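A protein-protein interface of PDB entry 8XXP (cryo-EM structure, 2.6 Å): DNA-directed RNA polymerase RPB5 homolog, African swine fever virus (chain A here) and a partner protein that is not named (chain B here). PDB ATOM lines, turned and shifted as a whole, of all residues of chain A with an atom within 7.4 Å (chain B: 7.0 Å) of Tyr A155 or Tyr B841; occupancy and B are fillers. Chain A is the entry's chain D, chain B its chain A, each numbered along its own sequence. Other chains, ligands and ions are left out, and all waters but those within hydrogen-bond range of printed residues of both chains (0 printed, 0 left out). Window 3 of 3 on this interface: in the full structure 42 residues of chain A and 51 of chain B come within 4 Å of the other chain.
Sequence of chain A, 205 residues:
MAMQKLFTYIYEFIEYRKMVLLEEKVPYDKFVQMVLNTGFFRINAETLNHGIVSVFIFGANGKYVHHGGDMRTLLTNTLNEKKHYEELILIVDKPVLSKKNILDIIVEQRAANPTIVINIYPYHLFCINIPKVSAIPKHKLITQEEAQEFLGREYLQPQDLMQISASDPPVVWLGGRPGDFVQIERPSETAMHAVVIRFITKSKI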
ATOM      1  N   GLU A 149      30.625   3.866  17.622  1.00  0.00           N
ATOM      2  CA  GLU A 149      29.692   4.974  17.456  1.00  0.00           C
ATOM      3  C   GLU A 149      28.249   4.511  17.624  1.00  0.00           C
ATOM      4  O   GLU A 149      27.419   5.246  18.174  1.00  0.00           O
ATOM      5  CB  GLU A 149      29.902   5.658  16.104  1.00  0.00           C
ATOM      6  CG  GLU A 149      29.614   4.808  14.894  1.00  0.00           C
ATOM      7  CD  GLU A 149      28.327   5.199  14.198  1.00  0.00           C
ATOM      8  OE1 GLU A 149      27.917   6.371  14.327  1.00  0.00           O
ATOM      9  OE2 GLU A 149      27.724   4.335  13.526  1.00  0.00           O
ATOM     10  N   PHE A 150      27.933   3.292  17.177  1.00  0.00           N
ATOM     11  CA  PHE A 150      26.596   2.750  17.389  1.00  0.00           C
ATOM     12  C   PHE A 150      26.304   2.569  18.871  1.00  0.00           C
ATOM     13  O   PHE A 150      25.208   2.889  19.339  1.00  0.00           O
ATOM     14  CB  PHE A 150      26.449   1.423  16.645  1.00  0.00           C
ATOM     15  CG  PHE A 150      25.296   0.584  17.115  1.00  0.00           C
ATOM     16  CD1 PHE A 150      24.011   0.850  16.686  1.00  0.00           C
ATOM     17  CD2 PHE A 150      25.499  -0.479  17.976  1.00  0.00           C
ATOM     18  CE1 PHE A 150      22.956   0.079  17.112  1.00  0.00           C
ATOM     19  CE2 PHE A 150      24.444  -1.248  18.407  1.00  0.00           C
ATOM     20  CZ  PHE A 150      23.173  -0.971  17.973  1.00  0.00           C
ATOM     21  N   LEU A 151      27.273   2.053  19.627  1.00  0.00           N
ATOM     22  CA  LEU A 151      27.073   1.841  21.055  1.00  0.00           C
ATOM     23  C   LEU A 151      27.034   3.161  21.810  1.00  0.00           C
ATOM     24  O   LEU A 151      26.333   3.284  22.818  1.00  0.00           O
ATOM     25  CB  LEU A 151      28.171   0.939  21.609  1.00  0.00           C
ATOM     26  CG  LEU A 151      28.156  -0.535  21.215  1.00  0.00           C
ATOM     27  CD1 LEU A 151      29.388  -1.214  21.746  1.00  0.00           C
ATOM     28  CD2 LEU A 151      26.914  -1.213  21.731  1.00  0.00           C
ATOM     29  N   GLY A 152      27.805   4.149  21.358  1.00  0.00           N
ATOM     30  CA  GLY A 152      27.760   5.452  21.991  1.00  0.00           C
ATOM     31  C   GLY A 152      26.436   6.152  21.778  1.00  0.00           C
ATOM     32  O   GLY A 152      25.904   6.783  22.694  1.00  0.00           O
ATOM     33  N   ARG A 153      25.887   6.055  20.567  1.00  0.00           N
ATOM     34  CA  ARG A 153      24.576   6.635  20.312  1.00  0.00           C
ATOM     35  C   ARG A 153      23.484   5.927  21.100  1.00  0.00           C
ATOM     36  O   ARG A 153      22.510   6.560  21.516  1.00  0.00           O
ATOM     37  CB  ARG A 153      24.270   6.591  18.819  1.00  0.00           C
ATOM     38  CG  ARG A 153      23.057   7.387  18.411  1.00  0.00           C
ATOM     39  CD  ARG A 153      21.902   6.486  18.044  1.00  0.00           C
ATOM     40  NE  ARG A 153      20.666   7.241  17.893  1.00  0.00           N
ATOM     41  CZ  ARG A 153      19.456   6.735  18.071  1.00  0.00           C
ATOM     42  NH1 ARG A 153      19.281   5.463  18.380  1.00  0.00           N
ATOM     43  NH2 ARG A 153      18.396   7.524  17.936  1.00  0.00           N
ATOM     44  N   GLU A 154      23.627   4.627  21.313  1.00  0.00           N
ATOM     45  CA  GLU A 154      22.625   3.822  21.995  1.00  0.00           C
ATOM     46  C   GLU A 154      22.871   3.703  23.488  1.00  0.00           C
ATOM     47  O   GLU A 154      22.043   3.107  24.184  1.00  0.00           O
ATOM     48  CB  GLU A 154      22.578   2.422  21.385  1.00  0.00           C
ATOM     49  CG  GLU A 154      22.172   2.383  19.933  1.00  0.00           C
ATOM     50  CD  GLU A 154      20.679   2.422  19.747  1.00  0.00           C
ATOM     51  OE1 GLU A 154      19.998   1.497  20.232  1.00  0.00           O
ATOM     52  OE2 GLU A 154      20.186   3.373  19.108  1.00  0.00           O
ATOM     53  N   TYR A 155      23.978   4.244  23.993  1.00  0.00           N
ATOM     54  CA  TYR A 155      24.333   4.154  25.409  1.00  0.00           C
ATOM     55  C   TYR A 155      24.378   2.704  25.877  1.00  0.00           C
ATOM     56  O   TYR A 155      23.837   2.341  26.921  1.00  0.00           O
ATOM     57  CB  TYR A 155      23.368   4.973  26.259  1.00  0.00           C
ATOM     58  CG  TYR A 155      23.736   6.426  26.377  1.00  0.00           C
ATOM     59  CD1 TYR A 155      24.702   6.839  27.275  1.00  0.00           C
ATOM     60  CD2 TYR A 155      23.145   7.379  25.568  1.00  0.00           C
ATOM     61  CE1 TYR A 155      25.043   8.164  27.386  1.00  0.00           C
ATOM     62  CE2 TYR A 155      23.477   8.705  25.678  1.00  0.00           C
ATOM     63  CZ  TYR A 155      24.429   9.091  26.587  1.00  0.00           C
ATOM     64  OH  TYR A 155      24.773  10.414  26.693  1.00  0.00           O
ATOM     65  N   LEU A 156      25.038   1.864  25.090  1.00  0.00           N
ATOM     66  CA  LEU A 156      25.112   0.438  25.361  1.00  0.00           C
ATOM     67  C   LEU A 156      26.560   0.006  25.516  1.00  0.00           C
ATOM     68  O   LEU A 156      27.454   0.538  24.855  1.00  0.00           O
ATOM     69  CB  LEU A 156      24.466  -0.378  24.242  1.00  0.00           C
ATOM     70  CG  LEU A 156      22.957  -0.300  24.055  1.00  0.00           C
ATOM     71  CD1 LEU A 156      22.585  -0.922  22.740  1.00  0.00           C
ATOM     72  CD2 LEU A 156      22.248  -0.997  25.183  1.00  0.00           C
ATOM     73  N   GLN A 157      26.780  -0.952  26.398  1.00  0.00           N
ATOM     74  CA  GLN A 157      28.029  -1.681  26.431  1.00  0.00           C
ATOM     75  C   GLN A 157      27.961  -2.833  25.438  1.00  0.00           C
ATOM     76  O   GLN A 157      26.875  -3.259  25.048  1.00  0.00           O
ATOM     77  CB  GLN A 157      28.293  -2.202  27.837  1.00  0.00           C
ATOM     78  CG  GLN A 157      29.354  -1.423  28.568  1.00  0.00           C
ATOM     79  CD  GLN A 157      28.896  -0.027  28.909  1.00  0.00           C
ATOM     80  OE1 GLN A 157      27.718   0.202  29.168  1.00  0.00           O
ATOM     81  NE2 GLN A 157      29.824   0.921  28.900  1.00  0.00           N
ATOM     82  N   ASP A 160      25.631  -5.639  26.460  1.00  0.00           N
ATOM     83  CA  ASP A 160      24.188  -5.472  26.383  1.00  0.00           C
ATOM     84  C   ASP A 160      23.608  -5.995  25.082  1.00  0.00           C
ATOM     85  O   ASP A 160      22.409  -6.275  25.022  1.00  0.00           O
ATOM     86  CB  ASP A 160      23.820  -3.997  26.530  1.00  0.00           C
ATOM     87  CG  ASP A 160      24.178  -3.441  27.885  1.00  0.00           C
ATOM     88  OD1 ASP A 160      24.405  -4.237  28.817  1.00  0.00           O
ATOM     89  OD2 ASP A 160      24.231  -2.204  28.018  1.00  0.00           O
ATOM     90  N   VAL B 838       9.886  -2.501  26.848  1.00  0.00           N
ATOM     91  CA  VAL B 838      10.316  -1.499  25.882  1.00  0.00           C
ATOM     92  C   VAL B 838      11.005  -0.359  26.614  1.00  0.00           C
ATOM     93  O   VAL B 838      10.452   0.211  27.561  1.00  0.00           O
ATOM     94  CB  VAL B 838       9.114  -0.993  25.072  1.00  0.00           C
ATOM     95  CG1 VAL B 838       9.479   0.235  24.276  1.00  0.00           C
ATOM     96  CG2 VAL B 838       8.598  -2.082  24.165  1.00  0.00           C
ATOM     97  N   ASP B 839      12.218  -0.020  26.184  1.00  0.00           N
ATOM     98  CA  ASP B 839      12.978   1.051  26.803  1.00  0.00           C
ATOM     99  C   ASP B 839      12.808   2.342  26.002  1.00  0.00           C
ATOM    100  O   ASP B 839      11.969   2.437  25.107  1.00  0.00           O
ATOM    101  CB  ASP B 839      14.446   0.648  26.956  1.00  0.00           C
ATOM    102  CG  ASP B 839      15.112   0.348  25.641  1.00  0.00           C
ATOM    103  OD1 ASP B 839      14.403   0.212  24.637  1.00  0.00           O
ATOM    104  OD2 ASP B 839      16.351   0.236  25.611  1.00  0.00           O
ATOM    105  N   TYR B 840      13.608   3.357  26.329  1.00  0.00           N
ATOM    106  CA  TYR B 840      13.447   4.671  25.718  1.00  0.00           C
ATOM    107  C   TYR B 840      13.910   4.728  24.273  1.00  0.00           C
ATOM    108  O   TYR B 840      13.634   5.722  23.598  1.00  0.00           O
ATOM    109  CB  TYR B 840      14.186   5.727  26.529  1.00  0.00           C
ATOM    110  CG  TYR B 840      13.543   6.004  27.856  1.00  0.00           C
ATOM    111  CD1 TYR B 840      12.238   6.449  27.929  1.00  0.00           C
ATOM    112  CD2 TYR B 840      14.240   5.822  29.033  1.00  0.00           C
ATOM    113  CE1 TYR B 840      11.645   6.696  29.137  1.00  0.00           C
ATOM    114  CE2 TYR B 840      13.657   6.068  30.242  1.00  0.00           C
ATOM    115  CZ  TYR B 840      12.361   6.507  30.290  1.00  0.00           C
ATOM    116  OH  TYR B 840      11.776   6.757  31.502  1.00  0.00           O
ATOM    117  N   TYR B 841      14.607   3.713  23.787  1.00  0.00           N
ATOM    118  CA  TYR B 841      14.936   3.623  22.375  1.00  0.00           C
ATOM    119  C   TYR B 841      13.934   2.780  21.614  1.00  0.00           C
ATOM    120  O   TYR B 841      14.115   2.563  20.413  1.00  0.00           O
ATOM    121  CB  TYR B 841      16.335   3.038  22.194  1.00  0.00           C
ATOM    122  CG  TYR B 841      17.446   3.949  22.640  1.00  0.00           C
ATOM    123  CD1 TYR B 841      17.680   4.181  23.984  1.00  0.00           C
ATOM    124  CD2 TYR B 841      18.272   4.562  21.717  1.00  0.00           C
ATOM    125  CE1 TYR B 841      18.692   5.004  24.394  1.00  0.00           C
ATOM    126  CE2 TYR B 841      19.290   5.389  22.119  1.00  0.00           C
ATOM    127  CZ  TYR B 841      19.496   5.605  23.459  1.00  0.00           C
ATOM    128  OH  TYR B 841      20.509   6.429  23.868  1.00  0.00           O
ATOM    129  N   ARG B 842      12.892   2.306  22.291  1.00  0.00           N
ATOM    130  CA  ARG B 842      11.918   1.352  21.777  1.00  0.00           C
ATOM    131  C   ARG B 842      12.551   0.012  21.442  1.00  0.00           C
ATOM    132  O   ARG B 842      11.962  -0.796  20.724  1.00  0.00           O
ATOM    133  CB  ARG B 842      11.156   1.915  20.579  1.00  0.00           C
ATOM    134  CG  ARG B 842      10.251   3.045  20.978  1.00  0.00           C
ATOM    135  CD  ARG B 842       9.263   3.411  19.909  1.00  0.00           C
ATOM    136  NE  ARG B 842       8.381   4.462  20.390  1.00  0.00           N
ATOM    137  CZ  ARG B 842       8.644   5.756  20.287  1.00  0.00           C
ATOM    138  NH1 ARG B 842       9.736   6.192  19.687  1.00  0.00           N
ATOM    139  NH2 ARG B 842       7.793   6.633  20.803  1.00  0.00           N
ATOM    140  N   ARG B 843      13.747  -0.236  21.960  1.00  0.00           N
ATOM    141  CA  ARG B 843      14.276  -1.583  22.002  1.00  0.00           C
ATOM    142  C   ARG B 843      13.537  -2.382  23.064  1.00  0.00           C
ATOM    143  O   ARG B 843      12.873  -1.832  23.942  1.00  0.00           O
ATOM    144  CB  ARG B 843      15.771  -1.566  22.314  1.00  0.00           C
ATOM    145  CG  ARG B 843      16.551  -0.530  21.548  1.00  0.00           C
ATOM    146  CD  ARG B 843      17.988  -0.454  22.011  1.00  0.00           C
ATOM    147  NE  ARG B 843      18.089  -0.166  23.434  1.00  0.00           N
ATOM    148  CZ  ARG B 843      18.945   0.693  23.964  1.00  0.00           C
ATOM    149  NH1 ARG B 843      19.797   1.369  23.217  1.00  0.00           N
ATOM    150  NH2 ARG B 843      18.942   0.882  25.278  1.00  0.00           N
ATOM    151  N   VAL B 844      13.645  -3.697  22.980  1.00  0.00           N
ATOM    152  CA  VAL B 844      13.162  -4.571  24.037  1.00  0.00           C
ATOM    153  C   VAL B 844      14.379  -5.161  24.721  1.00  0.00           C
ATOM    154  O   VAL B 844      15.238  -5.763  24.069  1.00  0.00           O
ATOM    155  CB  VAL B 844      12.232  -5.664  23.507  1.00  0.00           C
ATOM    156  CG1 VAL B 844      11.581  -6.360  24.661  1.00  0.00           C
ATOM    157  CG2 VAL B 844      11.190  -5.055  22.610  1.00  0.00           C
ATOM    158  N   GLN B 853      16.324  -5.022  18.848  1.00  0.00           N
ATOM    159  CA  GLN B 853      16.787  -3.672  18.550  1.00  0.00           C
ATOM    160  C   GLN B 853      15.623  -2.703  18.404  1.00  0.00           C
ATOM    161  O   GLN B 853      15.753  -1.523  18.736  1.00  0.00           O
ATOM    162  CB  GLN B 853      17.637  -3.681  17.284  1.00  0.00           C
ATOM    163  CG  GLN B 853      18.388  -2.402  17.029  1.00  0.00           C
ATOM    164  CD  GLN B 853      19.385  -2.077  18.111  1.00  0.00           C
ATOM    165  OE1 GLN B 853      20.286  -2.861  18.393  1.00  0.00           O
ATOM    166  NE2 GLN B 853      19.236  -0.914  18.720  1.00  0.00           N
ATOM    167  N   LEU B 854      14.496  -3.173  17.885  1.00  0.00           N
ATOM    168  CA  LEU B 854      13.263  -2.410  17.846  1.00  0.00           C
ATOM    169  C   LEU B 854      12.128  -3.393  18.053  1.00  0.00           C
ATOM    170  O   LEU B 854      12.205  -4.534  17.601  1.00  0.00           O
ATOM    171  CB  LEU B 854      13.111  -1.648  16.529  1.00  0.00           C
ATOM    172  CG  LEU B 854      12.250  -0.392  16.547  1.00  0.00           C
ATOM    173  CD1 LEU B 854      12.871   0.687  17.397  1.00  0.00           C
ATOM    174  CD2 LEU B 854      12.080   0.097  15.147  1.00  0.00           C
ATOM    175  N   TYR B 855      11.075  -2.945  18.734  1.00  0.00           N
ATOM    176  CA  TYR B 855      10.107  -3.871  19.312  1.00  0.00           C
ATOM    177  C   TYR B 855       9.514  -4.825  18.281  1.00  0.00           C
ATOM    178  O   TYR B 855       9.730  -6.036  18.364  1.00  0.00           O
ATOM    179  CB  TYR B 855       8.991  -3.106  20.027  1.00  0.00           C
ATOM    180  CG  TYR B 855       7.740  -3.926  20.235  1.00  0.00           C
ATOM    181  CD1 TYR B 855       7.794  -5.163  20.854  1.00  0.00           C
ATOM    182  CD2 TYR B 855       6.510  -3.466  19.807  1.00  0.00           C
ATOM    183  CE1 TYR B 855       6.669  -5.913  21.028  1.00  0.00           C
ATOM    184  CE2 TYR B 855       5.376  -4.212  19.986  1.00  0.00           C
ATOM    185  CZ  TYR B 855       5.462  -5.434  20.600  1.00  0.00           C
ATOM    186  OH  TYR B 855       4.335  -6.188  20.788  1.00  0.00           O
ATOM    187  N   PHE B 975      10.844   7.977  14.830  1.00  0.00           N
ATOM    188  CA  PHE B 975      11.386   7.117  15.864  1.00  0.00           C
ATOM    189  C   PHE B 975      12.317   7.855  16.807  1.00  0.00           C
ATOM    190  O   PHE B 975      12.734   7.274  17.811  1.00  0.00           O
ATOM    191  CB  PHE B 975      12.130   5.943  15.237  1.00  0.00           C
ATOM    192  CG  PHE B 975      11.249   5.008  14.482  1.00  0.00           C
ATOM    193  CD1 PHE B 975      10.371   4.180  15.146  1.00  0.00           C
ATOM    194  CD2 PHE B 975      11.299   4.952  13.105  1.00  0.00           C
ATOM    195  CE1 PHE B 975       9.558   3.323  14.451  1.00  0.00           C
ATOM    196  CE2 PHE B 975      10.490   4.095  12.413  1.00  0.00           C
ATOM    197  CZ  PHE B 975       9.620   3.279  13.087  1.00  0.00           C
ATOM    198  N   TYR B 990      19.374   0.753  11.645  1.00  0.00           N
ATOM    199  CA  TYR B 990      18.193  -0.017  12.007  1.00  0.00           C
ATOM    200  C   TYR B 990      16.939   0.847  12.026  1.00  0.00           C
ATOM    201  O   TYR B 990      15.839   0.337  11.802  1.00  0.00           O
ATOM    202  CB  TYR B 990      18.404  -0.703  13.356  1.00  0.00           C
ATOM    203  CG  TYR B 990      18.255   0.185  14.565  1.00  0.00           C
ATOM    204  CD1 TYR B 990      19.307   0.958  15.015  1.00  0.00           C
ATOM    205  CD2 TYR B 990      17.066   0.227  15.274  1.00  0.00           C
ATOM    206  CE1 TYR B 990      19.178   1.756  16.124  1.00  0.00           C
ATOM    207  CE2 TYR B 990      16.927   1.021  16.379  1.00  0.00           C
ATOM    208  CZ  TYR B 990      17.985   1.785  16.801  1.00  0.00           C
ATOM    209  OH  TYR B 990      17.850   2.583  17.909  1.00  0.00           O
ATOM    210  N   LEU B 991      17.080   2.144  12.298  1.00  0.00           N
ATOM    211  CA  LEU B 991      15.933   3.040  12.247  1.00  0.00           C
ATOM    212  C   LEU B 991      15.567   3.417  10.821  1.00  0.00           C
ATOM    213  O   LEU B 991      14.405   3.725  10.548  1.00  0.00           O
ATOM    214  CB  LEU B 991      16.201   4.298  13.064  1.00  0.00           C
ATOM    215  CG  LEU B 991      16.058   4.152  14.573  1.00  0.00           C
ATOM    216  CD1 LEU B 991      16.084   5.513  15.216  1.00  0.00           C
ATOM    217  CD2 LEU B 991      14.785   3.414  14.924  1.00  0.00           C
ATOM    218  N   TYR B1037       7.071   3.746  25.717  1.00  0.00           N
ATOM    219  CA  TYR B1037       8.166   3.393  26.601  1.00  0.00           C
ATOM    220  C   TYR B1037       7.633   2.728  27.859  1.00  0.00           C
ATOM    221  O   TYR B1037       6.673   3.200  28.471  1.00  0.00           O
ATOM    222  CB  TYR B1037       8.959   4.635  26.975  1.00  0.00           C
ATOM    223  CG  TYR B1037       9.457   5.426  25.799  1.00  0.00           C
ATOM    224  CD1 TYR B1037      10.019   4.795  24.707  1.00  0.00           C
ATOM    225  CD2 TYR B1037       9.367   6.806  25.781  1.00  0.00           C
ATOM    226  CE1 TYR B1037      10.482   5.512  23.638  1.00  0.00           C
ATOM    227  CE2 TYR B1037       9.825   7.530  24.711  1.00  0.00           C
ATOM    228  CZ  TYR B1037      10.382   6.877  23.646  1.00  0.00           C
ATOM    229  OH  TYR B1037      10.847   7.590  22.574  1.00  0.00           O
ATOM    230  N   TYR B1426       7.392   3.975  34.529  1.00  0.00           N
ATOM    231  CA  TYR B1426       8.626   3.868  33.768  1.00  0.00           C
ATOM    232  C   TYR B1426       9.420   5.164  33.807  1.00  0.00           C
ATOM    233  O   TYR B1426      10.638   5.152  34.014  1.00  0.00           O
ATOM    234  CB  TYR B1426       8.332   3.465  32.327  1.00  0.00           C
ATOM    235  CG  TYR B1426       9.568   2.988  31.631  1.00  0.00           C
ATOM    236  CD1 TYR B1426      10.121   1.759  31.940  1.00  0.00           C
ATOM    237  CD2 TYR B1426      10.208   3.778  30.694  1.00  0.00           C
ATOM    238  CE1 TYR B1426      11.259   1.324  31.324  1.00  0.00           C
ATOM    239  CE2 TYR B1426      11.349   3.347  30.071  1.00  0.00           C
ATOM    240  CZ  TYR B1426      11.871   2.122  30.393  1.00  0.00           C
ATOM    241  OH  TYR B1426      13.012   1.682  29.784  1.00  0.00           O
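OD2 of Asp B839 is in salt-bridge range of NH2 of Arg B843 (2.7 Å).
The backbone carbonyl oxygen of Leu A151 lies within hydrogen-bond range of the backbone NH of Leu A156, 3.0 Å away.
Hydrophobic or aromatic side chains of chain B within 4 Å of the printed part of chain A: Tyr B841 and Tyr B990.
Hydrophobic or aromatic side chains of chain A that line the printed part of chain B: Phe A150, Tyr A155 and Leu A156.
Along chain A the printed residues that touch a printed residue of chain B span positions 150 to 156.
Printed residues of chain B within 4 Å of Tyr A155: Tyr B841.
Of chain A, only Arg A153 (3.1 Å), Glu A154 (3.4 Å) and Tyr A155 (3.3 Å) come within 4 Å of Tyr B841.
Printed residues of chain B within 4 Å of Glu A154: Tyr B841 (3.4 Å), Arg B843 (3.0 Å), Gln B853 (2.9 Å) and Tyr B990 (2.7 Å).
Printed residues of chain A within 4 Å of Gln B853: Phe A150 and Glu A154.
Leu B991 touches none of the printed residues of chain A.
Leu B854 touches none of the printed residues of chain A.
The nearest residue of chain B that does not touch Tyr A155 is Arg B843 (5.1 Å).
The nearest residue of chain A that does not touch Tyr B841 is Gly A152 (5.5 Å).
The nearest printed residue of chain B that does not touch Arg A153 is Leu B991 (4.1 Å).
The side-chain hydroxyl (OH) of Tyr B990 lies within hydrogen-bond range of the guanidinium group (NH1) of Arg A153, at 3.3 Å.
The side-chain carboxylate (OE1) of Glu A154 is in hydrogen-bond range of the side-chain amide nitrogen (NE2) of Gln B853, at 2.9 Å.
The guanidinium group (NH1) of Arg B843 is in salt-bridge range of the side-chain carboxylate (OE1) of Glu A154.
The side-chain hydroxyl (OH) of Tyr B990 sits at hydrogen-bond distance from the side-chain carboxylate (OE2) of Glu A154 (2.7 Å).
OH of Tyr B841 is in hydrogen-bond range of O of Arg A153, at 3.1 Å.
Gln B853 touches Phe A150.
Tyr B841 touches Glu A154.
CD2 of Tyr A155 touches OH of Tyr B841, at 3.3 Å.
Arg B843 touches Leu A156 (NH1 to CD1, 3.6 Å).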
